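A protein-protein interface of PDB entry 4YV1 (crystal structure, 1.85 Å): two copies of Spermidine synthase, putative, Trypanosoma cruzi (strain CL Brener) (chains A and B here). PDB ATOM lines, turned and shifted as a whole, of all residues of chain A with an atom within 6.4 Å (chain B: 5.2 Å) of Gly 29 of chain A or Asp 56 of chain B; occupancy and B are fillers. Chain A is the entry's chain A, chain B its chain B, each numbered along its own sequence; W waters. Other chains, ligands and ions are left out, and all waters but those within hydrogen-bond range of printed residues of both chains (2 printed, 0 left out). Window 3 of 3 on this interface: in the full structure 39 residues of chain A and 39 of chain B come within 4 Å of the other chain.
The side-chain carboxylate (OD2) of Asp 56 of chain B is in salt-bridge range of the guanidinium group (NH1) of Arg 35 of chain B, 2.8 Å away.
OD1 of Asp 56 of chain B is in hydrogen-bond range of N of Lys 58 of chain B (2.7 Å).
Among the printed residues, pairs that only touch across the chains: Glu 23 of chain A with Trp 19 of chain B (3.6 Å), Pro 28 of chain A with Lys 58 of chain B (3.4 Å), Pro 28 of chain A with Gly 59 of chain B (3.7 Å), Gly 29 of chain A with Trp 19 of chain B (3.5 Å), Gly 29 of chain A with Leu 34 of chain B (3.4 Å), Gly 29 of chain A with Asp 56 of chain B (3.7 Å), Gln 30 of chain A with Trp 19 of chain B (3.8 Å), Gln 30 of chain A with Ser 33 of chain B (3.4 Å), Gln 30 of chain A with Leu 34 of chain B (3.7 Å) and Ala 31 of chain A with Trp 19 of chain B (3.97 Å).
Gly 29 of chain A touches four residues of chain B.
Printed residues of chain A within 4 Å of Asp 56 of chain B: Gly 29.
Printed residues of chain B within 4 Å of Gln 30 of chain A: Trp 19, Ser 33 and Leu 34.
Of the printed residues of chain A, Lys 58 of chain B touches Pro 28 (3.4 Å).
Of the printed residues of chain B, Pro 28 of chain A touches Lys 58 and Gly 59.
The nearest residue of chain B that does not touch Gly 29 of chain A is Ser 33 of chain B (4.1 Å).
The nearest printed residue of chain A that does not touch Asp 56 of chain B is Pro 28 of chain A (4.01 Å).
The nearest printed residue of chain B that does not touch Ala 31 of chain A is Leu 34 of chain B (5.1 Å).
No position is printed for both chains.
Of the 12 pairs that touch across the chains among the printed residues, none has its exchanged pair printed and touching as well.
The backbone carbonyl oxygen of Gly 29 of chain A lies within hydrogen-bond range of the backbone NH of Arg 35 of chain B (2.9 Å).
The backbone NH (N) of Ser 33 of chain B sits at hydrogen-bond distance from the backbone carbonyl oxygen (O) of Ala 31 of chain A (2.9 Å).
Along chain A the printed residues that touch a printed residue of chain B span positions 23 to 31.
Of the 13 printed residues of chain B, 7 touch a printed residue of chain A.
Hydrophobic or aromatic side chains of chain B within 4 Å of the printed part of chain A: Trp 19 and Leu 34.
Among the printed residues, no Asp or Glu carboxylate lies within 4 Å of a Lys or Arg side-chain nitrogen of the other chain.
Water W2 lies within hydrogen-bond range of N of Asp 56 of chain B (2.8 Å), O of Arg 35 of chain B (2.9 Å) and O of Gly 29 of chain A (2.9 Å).
Water W1 lies within hydrogen-bond range of OG of Ser 33 of chain B (3.1 Å) and O of Ala 31 of chain A (3.5 Å).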
ATOM      1  N   GLU A  23     -28.566  15.094 -23.561  1.00  0.00           N
ATOM      2  CA  GLU A  23     -27.559  16.151 -23.605  1.00  0.00           C
ATOM      3  C   GLU A  23     -27.826  16.958 -24.837  1.00  0.00           C
ATOM      4  O   GLU A  23     -28.022  16.397 -25.911  1.00  0.00           O
ATOM      5  CB  GLU A  23     -26.086  15.663 -23.566  1.00  0.00           C
ATOM      6  CG  GLU A  23     -25.579  14.662 -24.597  1.00  0.00           C
ATOM      7  CD  GLU A  23     -24.160  14.132 -24.283  1.00  0.00           C
ATOM      8  OE1 GLU A  23     -23.152  14.844 -24.498  1.00  0.00           O
ATOM      9  OE2 GLU A  23     -24.047  12.971 -23.832  1.00  0.00           O
ATOM     10  N   ASN A  24     -27.882  18.274 -24.681  1.00  0.00           N
ATOM     11  CA  ASN A  24     -28.137  19.139 -25.832  1.00  0.00           C
ATOM     12  C   ASN A  24     -26.893  19.775 -26.418  1.00  0.00           C
ATOM     13  O   ASN A  24     -25.962  20.140 -25.690  1.00  0.00           O
ATOM     14  CB  ASN A  24     -29.203  20.187 -25.524  1.00  0.00           C
ATOM     15  CG  ASN A  24     -30.617  19.651 -25.706  1.00  0.00           C
ATOM     16  OD1 ASN A  24     -30.815  18.493 -26.104  1.00  0.00           O
ATOM     17  ND2 ASN A  24     -31.611  20.492 -25.420  1.00  0.00           N
ATOM     18  N   TRP A  27     -25.968  23.209 -25.143  1.00  0.00           N
ATOM     19  CA  TRP A  27     -25.290  23.244 -23.840  1.00  0.00           C
ATOM     20  C   TRP A  27     -24.262  22.105 -23.652  1.00  0.00           C
ATOM     21  O   TRP A  27     -24.569  21.046 -23.097  1.00  0.00           O
ATOM     22  CB  TRP A  27     -26.263  23.383 -22.659  1.00  0.00           C
ATOM     23  CG  TRP A  27     -27.622  22.714 -22.744  1.00  0.00           C
ATOM     24  CD1 TRP A  27     -27.918  21.405 -22.448  1.00  0.00           C
ATOM     25  CD2 TRP A  27     -28.881  23.350 -23.058  1.00  0.00           C
ATOM     26  NE1 TRP A  27     -29.278  21.182 -22.584  1.00  0.00           N
ATOM     27  CE2 TRP A  27     -29.892  22.353 -22.957  1.00  0.00           C
ATOM     28  CE3 TRP A  27     -29.250  24.659 -23.424  1.00  0.00           C
ATOM     29  CZ2 TRP A  27     -31.257  22.628 -23.214  1.00  0.00           C
ATOM     30  CZ3 TRP A  27     -30.603  24.936 -23.668  1.00  0.00           C
ATOM     31  CH2 TRP A  27     -31.589  23.919 -23.567  1.00  0.00           C
ATOM     32  N   PRO A  28     -23.028  22.336 -24.112  1.00  0.00           N
ATOM     33  CA  PRO A  28     -22.029  21.261 -24.284  1.00  0.00           C
ATOM     34  C   PRO A  28     -21.404  20.770 -22.965  1.00  0.00           C
ATOM     35  O   PRO A  28     -21.130  21.588 -22.093  1.00  0.00           O
ATOM     36  CB  PRO A  28     -20.964  21.907 -25.177  1.00  0.00           C
ATOM     37  CG  PRO A  28     -21.354  23.341 -25.341  1.00  0.00           C
ATOM     38  CD  PRO A  28     -22.473  23.661 -24.415  1.00  0.00           C
ATOM     39  N   GLY A  29     -21.179  19.452 -22.845  1.00  0.00           N
ATOM     40  CA  GLY A  29     -20.496  18.903 -21.692  1.00  0.00           C
ATOM     41  C   GLY A  29     -21.363  18.634 -20.454  1.00  0.00           C
ATOM     42  O   GLY A  29     -20.829  18.428 -19.388  1.00  0.00           O
ATOM     43  N   GLN A  30     -22.685  18.624 -20.603  1.00  0.00           N
ATOM     44  CA  GLN A  30     -23.599  18.273 -19.466  1.00  0.00           C
ATOM     45  C   GLN A  30     -24.692  17.333 -19.934  1.00  0.00           C
ATOM     46  O   GLN A  30     -25.138  17.431 -21.073  1.00  0.00           O
ATOM     47  CB  GLN A  30     -24.204  19.532 -18.809  1.00  0.00           C
ATOM     48  CG  GLN A  30     -25.036  20.433 -19.744  1.00  0.00           C
ATOM     49  CD  GLN A  30     -25.636  21.672 -19.020  1.00  0.00           C
ATOM     50  OE1 GLN A  30     -26.490  21.547 -18.127  1.00  0.00           O
ATOM     51  NE2 GLN A  30     -25.196  22.863 -19.420  1.00  0.00           N
ATOM     52  N   ALA A  31     -25.066  16.370 -19.081  1.00  0.00           N
ATOM     53  CA  ALA A  31     -26.112  15.370 -19.413  1.00  0.00           C
ATOM     54  C   ALA A  31     -26.955  15.001 -18.207  1.00  0.00           C
ATOM     55  O   ALA A  31     -26.474  15.088 -17.074  1.00  0.00           O
ATOM     56  CB  ALA A  31     -25.505  14.112 -19.978  1.00  0.00           C
ATOM     57  N   TRP B  19     -16.009  11.815 -17.979  1.00  0.00           N
ATOM     58  CA  TRP B  19     -17.228  12.447 -17.474  1.00  0.00           C
ATOM     59  C   TRP B  19     -17.359  12.131 -15.979  1.00  0.00           C
ATOM     60  O   TRP B  19     -17.223  10.965 -15.541  1.00  0.00           O
ATOM     61  CB  TRP B  19     -18.461  11.931 -18.193  1.00  0.00           C
ATOM     62  CG  TRP B  19     -18.648  12.466 -19.549  1.00  0.00           C
ATOM     63  CD1 TRP B  19     -17.889  12.169 -20.658  1.00  0.00           C
ATOM     64  CD2 TRP B  19     -19.640  13.434 -19.984  1.00  0.00           C
ATOM     65  NE1 TRP B  19     -18.341  12.869 -21.749  1.00  0.00           N
ATOM     66  CE2 TRP B  19     -19.412  13.656 -21.380  1.00  0.00           C
ATOM     67  CE3 TRP B  19     -20.722  14.112 -19.336  1.00  0.00           C
ATOM     68  CZ2 TRP B  19     -20.208  14.513 -22.148  1.00  0.00           C
ATOM     69  CZ3 TRP B  19     -21.471  15.017 -20.089  1.00  0.00           C
ATOM     70  CH2 TRP B  19     -21.231  15.184 -21.489  1.00  0.00           C
ATOM     71  N   SER B  33     -24.397  14.426 -15.181  1.00  0.00           N
ATOM     72  CA  SER B  33     -22.998  14.251 -15.607  1.00  0.00           C
ATOM     73  C   SER B  33     -22.465  15.525 -16.152  1.00  0.00           C
ATOM     74  O   SER B  33     -23.210  16.293 -16.770  1.00  0.00           O
ATOM     75  CB  SER B  33     -22.915  13.208 -16.727  1.00  0.00           C
ATOM     76  OG  SER B  33     -23.156  11.949 -16.209  1.00  0.00           O
ATOM     77  N   LEU B  34     -21.175  15.776 -15.880  1.00  0.00           N
ATOM     78  CA  LEU B  34     -20.421  16.864 -16.442  1.00  0.00           C
ATOM     79  C   LEU B  34     -19.119  16.279 -17.008  1.00  0.00           C
ATOM     80  O   LEU B  34     -18.404  15.538 -16.322  1.00  0.00           O
ATOM     81  CB  LEU B  34     -20.078  17.938 -15.377  1.00  0.00           C
ATOM     82  CG  LEU B  34     -21.219  18.774 -14.797  1.00  0.00           C
ATOM     83  CD1 LEU B  34     -20.695  19.668 -13.689  1.00  0.00           C
ATOM     84  CD2 LEU B  34     -21.878  19.645 -15.879  1.00  0.00           C
ATOM     85  N   ARG B  35     -18.810  16.644 -18.253  1.00  0.00           N
ATOM     86  CA  ARG B  35     -17.516  16.291 -18.844  1.00  0.00           C
ATOM     87  C   ARG B  35     -16.381  17.044 -18.088  1.00  0.00           C
ATOM     88  O   ARG B  35     -16.549  18.150 -17.639  1.00  0.00           O
ATOM     89  CB  ARG B  35     -17.503  16.639 -20.322  1.00  0.00           C
ATOM     90  CG  ARG B  35     -16.194  16.306 -21.017  1.00  0.00           C
ATOM     91  CD  ARG B  35     -16.134  17.004 -22.346  1.00  0.00           C
ATOM     92  NE  ARG B  35     -16.794  16.144 -23.278  1.00  0.00           N
ATOM     93  CZ  ARG B  35     -17.628  16.523 -24.225  1.00  0.00           C
ATOM     94  NH1 ARG B  35     -17.963  17.803 -24.389  1.00  0.00           N
ATOM     95  NH2 ARG B  35     -18.108  15.596 -25.033  1.00  0.00           N
ATOM     96  N   VAL B  36     -15.252  16.392 -17.905  1.00  0.00           N
ATOM     97  CA  VAL B  36     -14.124  16.978 -17.172  1.00  0.00           C
ATOM     98  C   VAL B  36     -13.104  17.577 -18.137  1.00  0.00           C
ATOM     99  O   VAL B  36     -12.624  16.876 -19.033  1.00  0.00           O
ATOM    100  CB  VAL B  36     -13.497  15.915 -16.283  1.00  0.00           C
ATOM    101  CG1 VAL B  36     -12.279  16.509 -15.560  1.00  0.00           C
ATOM    102  CG2 VAL B  36     -14.561  15.355 -15.322  1.00  0.00           C
ATOM    103  N   GLU B  37     -12.782  18.857 -18.024  1.00  0.00           N
ATOM    104  CA  GLU B  37     -11.748  19.417 -18.921  1.00  0.00           C
ATOM    105  C   GLU B  37     -10.391  19.228 -18.249  1.00  0.00           C
ATOM    106  O   GLU B  37      -9.425  18.793 -18.882  1.00  0.00           O
ATOM    107  CB  GLU B  37     -11.999  20.886 -19.214  1.00  0.00           C
ATOM    108  CG  GLU B  37     -10.790  21.606 -19.839  1.00  0.00           C
ATOM    109  CD  GLU B  37     -10.507  21.058 -21.250  1.00  0.00           C
ATOM    110  OE1 GLU B  37     -11.371  20.349 -21.813  1.00  0.00           O
ATOM    111  OE2 GLU B  37      -9.437  21.381 -21.802  1.00  0.00           O
ATOM    112  N   GLU B  54     -12.080  21.434 -13.515  1.00  0.00           N
ATOM    113  CA  GLU B  54     -12.589  22.356 -14.467  1.00  0.00           C
ATOM    114  C   GLU B  54     -13.569  21.651 -15.390  1.00  0.00           C
ATOM    115  O   GLU B  54     -13.204  20.635 -16.027  1.00  0.00           O
ATOM    116  CB  GLU B  54     -11.452  22.956 -15.309  1.00  0.00           C
ATOM    117  CG  GLU B  54     -10.570  23.893 -14.516  1.00  0.00           C
ATOM    118  CD  GLU B  54      -9.296  24.295 -15.254  1.00  0.00           C
ATOM    119  OE1 GLU B  54      -9.207  24.155 -16.502  1.00  0.00           O
ATOM    120  OE2 GLU B  54      -8.363  24.752 -14.574  1.00  0.00           O
ATOM    121  N   SER B  55     -14.787  22.188 -15.523  1.00  0.00           N
ATOM    122  CA  SER B  55     -15.787  21.496 -16.386  1.00  0.00           C
ATOM    123  C   SER B  55     -15.536  21.943 -17.819  1.00  0.00           C
ATOM    124  O   SER B  55     -14.618  22.725 -18.091  1.00  0.00           O
ATOM    125  CB  SER B  55     -17.255  21.798 -15.993  1.00  0.00           C
ATOM    126  OG  SER B  55     -17.494  23.235 -16.143  1.00  0.00           O
ATOM    127  N   ASP B  56     -16.370  21.494 -18.747  1.00  0.00           N
ATOM    128  CA  ASP B  56     -16.155  21.837 -20.188  1.00  0.00           C
ATOM    129  C   ASP B  56     -16.143  23.339 -20.378  1.00  0.00           C
ATOM    130  O   ASP B  56     -17.121  23.964 -20.055  1.00  0.00           O
ATOM    131  CB  ASP B  56     -17.304  21.238 -20.958  1.00  0.00           C
ATOM    132  CG  ASP B  56     -17.096  21.264 -22.452  1.00  0.00           C
ATOM    133  OD1 ASP B  56     -16.710  22.302 -22.987  1.00  0.00           O
ATOM    134  OD2 ASP B  56     -17.358  20.221 -23.056  1.00  0.00           O
ATOM    135  N   PRO B  57     -15.061  23.934 -20.959  1.00  0.00           N
ATOM    136  CA  PRO B  57     -15.069  25.415 -21.160  1.00  0.00           C
ATOM    137  C   PRO B  57     -16.088  25.908 -22.182  1.00  0.00           C
ATOM    138  O   PRO B  57     -16.284  27.091 -22.255  1.00  0.00           O
ATOM    139  CB  PRO B  57     -13.643  25.717 -21.659  1.00  0.00           C
ATOM    140  CG  PRO B  57     -13.231  24.427 -22.335  1.00  0.00           C
ATOM    141  CD  PRO B  57     -13.828  23.323 -21.488  1.00  0.00           C
ATOM    142  N   LYS B  58     -16.711  25.002 -22.964  1.00  0.00           N
ATOM    143  CA  LYS B  58     -17.822  25.357 -23.835  1.00  0.00           C
ATOM    144  C   LYS B  58     -19.152  25.437 -23.020  1.00  0.00           C
ATOM    145  O   LYS B  58     -20.134  25.957 -23.501  1.00  0.00           O
ATOM    146  CB  LYS B  58     -17.948  24.395 -25.046  1.00  0.00           C
ATOM    147  CG  LYS B  58     -16.717  24.321 -25.969  1.00  0.00           C
ATOM    148  CD  LYS B  58     -16.376  25.677 -26.577  1.00  0.00           C
ATOM    149  CE  LYS B  58     -15.028  25.652 -27.302  1.00  0.00           C
ATOM    150  NZ  LYS B  58     -13.839  25.996 -26.450  1.00  0.00           N
ATOM    151  N   GLY B  59     -19.139  24.961 -21.765  1.00  0.00           N
ATOM    152  CA  GLY B  59     -20.307  25.032 -20.865  1.00  0.00           C
ATOM    153  C   GLY B  59     -20.060  26.148 -19.845  1.00  0.00           C
ATOM    154  O   GLY B  59     -18.999  26.766 -19.851  1.00  0.00           O
ATOM    155  N   PRO B  60     -21.077  26.469 -19.039  1.00  0.00           N
ATOM    156  CA  PRO B  60     -21.019  27.679 -18.202  1.00  0.00           C
ATOM    157  C   PRO B  60     -20.432  27.467 -16.799  1.00  0.00           C
ATOM    158  O   PRO B  60     -20.184  28.447 -16.087  1.00  0.00           O
ATOM    159  CB  PRO B  60     -22.512  28.033 -18.040  1.00  0.00           C
ATOM    160  CG  PRO B  60     -23.212  26.692 -18.119  1.00  0.00           C
ATOM    161  CD  PRO B  60     -22.458  25.936 -19.180  1.00  0.00           C
HETATM  162  O   HOH W   1     -26.107  11.644 -16.935  1.00  0.00           O
HETATM  163  O   HOH W   2     -18.684  19.997 -18.158  1.00  0.00           O
